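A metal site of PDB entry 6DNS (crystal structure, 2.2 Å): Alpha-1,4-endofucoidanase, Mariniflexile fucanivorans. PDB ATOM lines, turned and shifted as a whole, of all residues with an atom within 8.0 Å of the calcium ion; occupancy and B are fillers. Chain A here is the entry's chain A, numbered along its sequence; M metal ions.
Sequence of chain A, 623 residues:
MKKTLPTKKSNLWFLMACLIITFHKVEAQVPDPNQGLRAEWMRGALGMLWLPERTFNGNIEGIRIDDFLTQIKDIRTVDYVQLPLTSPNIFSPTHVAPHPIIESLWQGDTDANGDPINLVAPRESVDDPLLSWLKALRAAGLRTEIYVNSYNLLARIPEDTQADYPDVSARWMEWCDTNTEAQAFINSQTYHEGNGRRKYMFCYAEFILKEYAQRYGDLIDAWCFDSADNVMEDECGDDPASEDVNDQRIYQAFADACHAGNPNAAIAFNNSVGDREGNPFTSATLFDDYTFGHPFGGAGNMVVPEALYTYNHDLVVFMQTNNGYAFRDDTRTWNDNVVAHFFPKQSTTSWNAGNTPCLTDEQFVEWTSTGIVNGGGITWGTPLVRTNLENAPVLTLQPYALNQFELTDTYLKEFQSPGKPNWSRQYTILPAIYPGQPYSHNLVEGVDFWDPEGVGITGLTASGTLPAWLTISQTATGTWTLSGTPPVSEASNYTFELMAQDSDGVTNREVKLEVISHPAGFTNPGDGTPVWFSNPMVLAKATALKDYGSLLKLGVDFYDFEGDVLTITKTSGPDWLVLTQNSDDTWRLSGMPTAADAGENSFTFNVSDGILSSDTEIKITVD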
ATOM      1  N   SER A 417     -17.488   3.740 -15.002  1.00  0.00           N
ATOM      2  CA  SER A 417     -18.295   4.957 -14.930  1.00  0.00           C
ATOM      3  C   SER A 417     -17.423   6.153 -14.558  1.00  0.00           C
ATOM      4  O   SER A 417     -17.418   6.573 -13.393  1.00  0.00           O
ATOM      5  CB  SER A 417     -19.439   4.776 -13.929  1.00  0.00           C
ATOM      6  OG  SER A 417     -20.351   3.795 -14.372  1.00  0.00           O
ATOM      7  N   PRO A 418     -16.668   6.709 -15.525  1.00  0.00           N
ATOM      8  CA  PRO A 418     -15.809   7.857 -15.238  1.00  0.00           C
ATOM      9  C   PRO A 418     -16.598   9.137 -14.971  1.00  0.00           C
ATOM     10  O   PRO A 418     -17.749   9.262 -15.402  1.00  0.00           O
ATOM     11  CB  PRO A 418     -14.943   8.002 -16.497  1.00  0.00           C
ATOM     12  CG  PRO A 418     -15.214   6.788 -17.330  1.00  0.00           C
ATOM     13  CD  PRO A 418     -16.578   6.318 -16.950  1.00  0.00           C
ATOM     14  N   GLY A 419     -15.980  10.070 -14.249  1.00  0.00           N
ATOM     15  CA  GLY A 419     -16.569  11.371 -13.936  1.00  0.00           C
ATOM     16  C   GLY A 419     -17.079  11.430 -12.517  1.00  0.00           C
ATOM     17  O   GLY A 419     -16.296  11.574 -11.584  1.00  0.00           O
ATOM     18  N   LYS A 420     -18.398  11.307 -12.356  1.00  0.00           N
ATOM     19  CA  LYS A 420     -19.027  11.422 -11.035  1.00  0.00           C
ATOM     20  C   LYS A 420     -18.712  10.203 -10.153  1.00  0.00           C
ATOM     21  O   LYS A 420     -18.322   9.158 -10.674  1.00  0.00           O
ATOM     22  CB  LYS A 420     -20.540  11.572 -11.175  1.00  0.00           C
ATOM     23  CG  LYS A 420     -20.995  12.842 -11.876  1.00  0.00           C
ATOM     24  CD  LYS A 420     -22.495  12.830 -12.092  1.00  0.00           C
ATOM     25  CE  LYS A 420     -23.047  14.213 -12.396  1.00  0.00           C
ATOM     26  NZ  LYS A 420     -22.579  14.750 -13.706  1.00  0.00           N
ATOM     27  N   PRO A 421     -18.864  10.336  -8.815  1.00  0.00           N
ATOM     28  CA  PRO A 421     -18.541   9.209  -7.927  1.00  0.00           C
ATOM     29  C   PRO A 421     -19.385   7.958  -8.177  1.00  0.00           C
ATOM     30  O   PRO A 421     -20.554   8.058  -8.540  1.00  0.00           O
ATOM     31  CB  PRO A 421     -18.843   9.772  -6.524  1.00  0.00           C
ATOM     32  CG  PRO A 421     -18.719  11.242  -6.671  1.00  0.00           C
ATOM     33  CD  PRO A 421     -19.283  11.526  -8.035  1.00  0.00           C
ATOM     34  N   ASN A 422     -18.764   6.798  -7.996  1.00  0.00           N
ATOM     35  CA  ASN A 422     -19.430   5.499  -8.123  1.00  0.00           C
ATOM     36  C   ASN A 422     -19.661   4.935  -6.728  1.00  0.00           C
ATOM     37  O   ASN A 422     -18.821   5.103  -5.850  1.00  0.00           O
ATOM     38  CB  ASN A 422     -18.575   4.530  -8.933  1.00  0.00           C
ATOM     39  CG  ASN A 422     -18.190   5.075 -10.303  1.00  0.00           C
ATOM     40  OD1 ASN A 422     -18.683   6.113 -10.744  1.00  0.00           O
ATOM     41  ND2 ASN A 422     -17.306   4.355 -10.988  1.00  0.00           N
ATOM     42  N   TRP A 450     -16.354   5.904  -4.134  1.00  0.00           N
ATOM     43  CA  TRP A 450     -15.042   6.384  -4.565  1.00  0.00           C
ATOM     44  C   TRP A 450     -15.111   7.323  -5.765  1.00  0.00           C
ATOM     45  O   TRP A 450     -16.105   7.346  -6.503  1.00  0.00           O
ATOM     46  CB  TRP A 450     -14.121   5.202  -4.911  1.00  0.00           C
ATOM     47  CG  TRP A 450     -14.637   4.360  -6.036  1.00  0.00           C
ATOM     48  CD1 TRP A 450     -14.411   4.543  -7.372  1.00  0.00           C
ATOM     49  CD2 TRP A 450     -15.459   3.191  -5.934  1.00  0.00           C
ATOM     50  NE1 TRP A 450     -15.044   3.571  -8.107  1.00  0.00           N
ATOM     51  CE2 TRP A 450     -15.706   2.732  -7.250  1.00  0.00           C
ATOM     52  CE3 TRP A 450     -16.028   2.495  -4.858  1.00  0.00           C
ATOM     53  CZ2 TRP A 450     -16.480   1.604  -7.514  1.00  0.00           C
ATOM     54  CZ3 TRP A 450     -16.811   1.369  -5.126  1.00  0.00           C
ATOM     55  CH2 TRP A 450     -17.021   0.932  -6.436  1.00  0.00           C
ATOM     56  N   ASP A 451     -14.043   8.108  -5.939  1.00  0.00           N
ATOM     57  CA  ASP A 451     -13.829   8.924  -7.121  1.00  0.00           C
ATOM     58  C   ASP A 451     -13.093   8.073  -8.159  1.00  0.00           C
ATOM     59  O   ASP A 451     -12.008   7.569  -7.863  1.00  0.00           O
ATOM     60  CB  ASP A 451     -12.999  10.164  -6.758  1.00  0.00           C
ATOM     61  CG  ASP A 451     -12.645  11.031  -7.964  1.00  0.00           C
ATOM     62  OD1 ASP A 451     -13.296  10.929  -9.023  1.00  0.00           O
ATOM     63  OD2 ASP A 451     -11.693  11.820  -7.844  1.00  0.00           O
ATOM     64  N   PRO A 452     -13.675   7.888  -9.368  1.00  0.00           N
ATOM     65  CA  PRO A 452     -12.995   7.129 -10.435  1.00  0.00           C
ATOM     66  C   PRO A 452     -11.599   7.651 -10.808  1.00  0.00           C
ATOM     67  O   PRO A 452     -10.677   6.844 -10.982  1.00  0.00           O
ATOM     68  CB  PRO A 452     -13.945   7.268 -11.628  1.00  0.00           C
ATOM     69  CG  PRO A 452     -15.281   7.439 -11.007  1.00  0.00           C
ATOM     70  CD  PRO A 452     -15.057   8.234  -9.762  1.00  0.00           C
ATOM     71  N   GLU A 453     -11.438   8.964 -10.921  1.00  0.00           N
ATOM     72  CA  GLU A 453     -10.166   9.575 -11.327  1.00  0.00           C
ATOM     73  C   GLU A 453      -9.091   9.554 -10.230  1.00  0.00           C
ATOM     74  O   GLU A 453      -7.909   9.735 -10.524  1.00  0.00           O
ATOM     75  CB  GLU A 453     -10.372  11.020 -11.825  1.00  0.00           C
ATOM     76  CG  GLU A 453     -10.944  11.138 -13.228  1.00  0.00           C
ATOM     77  CD  GLU A 453     -12.404  10.714 -13.331  1.00  0.00           C
ATOM     78  OE1 GLU A 453     -12.770  10.069 -14.345  1.00  0.00           O
ATOM     79  OE2 GLU A 453     -13.186  11.013 -12.412  1.00  0.00           O
ATOM     80  N   GLY A 454      -9.505   9.355  -8.982  1.00  0.00           N
ATOM     81  CA  GLY A 454      -8.583   9.260  -7.847  1.00  0.00           C
ATOM     82  C   GLY A 454      -8.158  10.583  -7.242  1.00  0.00           C
ATOM     83  O   GLY A 454      -7.107  10.656  -6.592  1.00  0.00           O
ATOM     84  N   VAL A 455      -8.971  11.633  -7.435  1.00  0.00           N
ATOM     85  CA  VAL A 455      -8.729  12.936  -6.817  1.00  0.00           C
ATOM     86  C   VAL A 455      -9.207  12.867  -5.363  1.00  0.00           C
ATOM     87  O   VAL A 455      -8.431  13.101  -4.440  1.00  0.00           O
ATOM     88  CB  VAL A 455      -9.445  14.093  -7.575  1.00  0.00           C
ATOM     89  CG1 VAL A 455      -9.151  15.440  -6.925  1.00  0.00           C
ATOM     90  CG2 VAL A 455      -9.016  14.114  -9.046  1.00  0.00           C
ATOM     91  N   GLY A 456     -10.480  12.531  -5.185  1.00  0.00           N
ATOM     92  CA  GLY A 456     -11.061  12.334  -3.857  1.00  0.00           C
ATOM     93  C   GLY A 456     -12.514  12.741  -3.750  1.00  0.00           C
ATOM     94  O   GLY A 456     -13.042  13.428  -4.620  1.00  0.00           O
ATOM     95  N   ILE A 457     -13.142  12.291  -2.669  1.00  0.00           N
ATOM     96  CA  ILE A 457     -14.528  12.647  -2.337  1.00  0.00           C
ATOM     97  C   ILE A 457     -14.495  13.966  -1.573  1.00  0.00           C
ATOM     98  O   ILE A 457     -13.874  14.049  -0.508  1.00  0.00           O
ATOM     99  CB  ILE A 457     -15.191  11.541  -1.488  1.00  0.00           C
ATOM    100  CG1 ILE A 457     -15.265  10.209  -2.267  1.00  0.00           C
ATOM    101  CG2 ILE A 457     -16.576  11.961  -0.994  1.00  0.00           C
ATOM    102  CD1 ILE A 457     -16.171  10.207  -3.477  1.00  0.00           C
ATOM    103  N   GLN A 501     -20.086  13.203  -3.384  1.00  0.00           N
ATOM    104  CA  GLN A 501     -19.728  14.340  -4.251  1.00  0.00           C
ATOM    105  C   GLN A 501     -18.228  14.388  -4.532  1.00  0.00           C
ATOM    106  O   GLN A 501     -17.422  14.040  -3.666  1.00  0.00           O
ATOM    107  CB  GLN A 501     -20.152  15.643  -3.566  1.00  0.00           C
ATOM    108  CG  GLN A 501     -20.164  16.869  -4.477  1.00  0.00           C
ATOM    109  CD  GLN A 501     -20.221  18.180  -3.721  1.00  0.00           C
ATOM    110  OE1 GLN A 501     -20.587  18.227  -2.541  1.00  0.00           O
ATOM    111  NE2 GLN A 501     -19.858  19.266  -4.397  1.00  0.00           N
ATOM    112  N   ASP A 502     -17.864  14.817  -5.733  1.00  0.00           N
ATOM    113  CA  ASP A 502     -16.475  15.158  -6.066  1.00  0.00           C
ATOM    114  C   ASP A 502     -16.420  16.349  -7.033  1.00  0.00           C
ATOM    115  O   ASP A 502     -17.451  16.983  -7.285  1.00  0.00           O
ATOM    116  CB  ASP A 502     -15.720  13.903  -6.590  1.00  0.00           C
ATOM    117  CG  ASP A 502     -16.199  13.427  -7.953  1.00  0.00           C
ATOM    118  OD1 ASP A 502     -16.943  14.129  -8.665  1.00  0.00           O
ATOM    119  OD2 ASP A 502     -15.815  12.296  -8.325  1.00  0.00           O
ATOM    120  N   SER A 503     -15.228  16.652  -7.558  1.00  0.00           N
ATOM    121  CA  SER A 503     -15.036  17.757  -8.517  1.00  0.00           C
ATOM    122  C   SER A 503     -15.958  17.682  -9.752  1.00  0.00           C
ATOM    123  O   SER A 503     -16.465  18.714 -10.193  1.00  0.00           O
ATOM    124  CB  SER A 503     -13.573  17.806  -8.972  1.00  0.00           C
ATOM    125  OG  SER A 503     -13.184  16.590  -9.593  1.00  0.00           O
ATOM    126  N   ASP A 504     -16.160  16.471 -10.272  1.00  0.00           N
ATOM    127  CA  ASP A 504     -16.987  16.283 -11.476  1.00  0.00           C
ATOM    128  C   ASP A 504     -18.490  16.418 -11.240  1.00  0.00           C
ATOM    129  O   ASP A 504     -19.211  16.855 -12.139  1.00  0.00           O
ATOM    130  CB  ASP A 504     -16.671  14.931 -12.128  1.00  0.00           C
ATOM    131  CG  ASP A 504     -15.267  14.875 -12.716  1.00  0.00           C
ATOM    132  OD1 ASP A 504     -14.451  14.055 -12.245  1.00  0.00           O
ATOM    133  OD2 ASP A 504     -14.986  15.662 -13.638  1.00  0.00           O
ATOM    134  N   GLY A 505     -18.971  16.031 -10.058  1.00  0.00           N
ATOM    135  CA  GLY A 505     -20.391  16.175  -9.735  1.00  0.00           C
ATOM    136  C   GLY A 505     -20.836  15.474  -8.455  1.00  0.00           C
ATOM    137  O   GLY A 505     -20.073  15.397  -7.494  1.00  0.00           O
HETATM  138 CA    CA M   1     -14.286  12.250 -10.646  1.00  0.00          CA
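OD2 of Asp 451 sits at hydrogen-bond distance from N of Val 455 (2.8 Å). The side-chain carboxylate (OD2) of Asp 451 sits at hydrogen-bond distance from the backbone NH (N) of Gly 454 (3.5 Å). The backbone NH of Gly 456 sits at hydrogen-bond distance from the side-chain carboxylate of Asp 451, 3.0 Å away. The side-chain carboxylate (OD1) of Asp 502 sits at hydrogen-bond distance from the backbone NH (N) of Gly 505 (3.1 Å).
Within 4 Å of the calcium ion: Gly 419, Asp 451, Glu 453, Asp 502 and Asp 504.
The calcium ion is bound by the side-chain carboxylate of Asp 451, the backbone carbonyl oxygen of Gly 419, the side-chain carboxylate of Asp 504, the side-chain carboxylate of Glu 453 and the side-chain carboxylate of Asp 502. The calcium ion has five donor atoms within binding distance.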
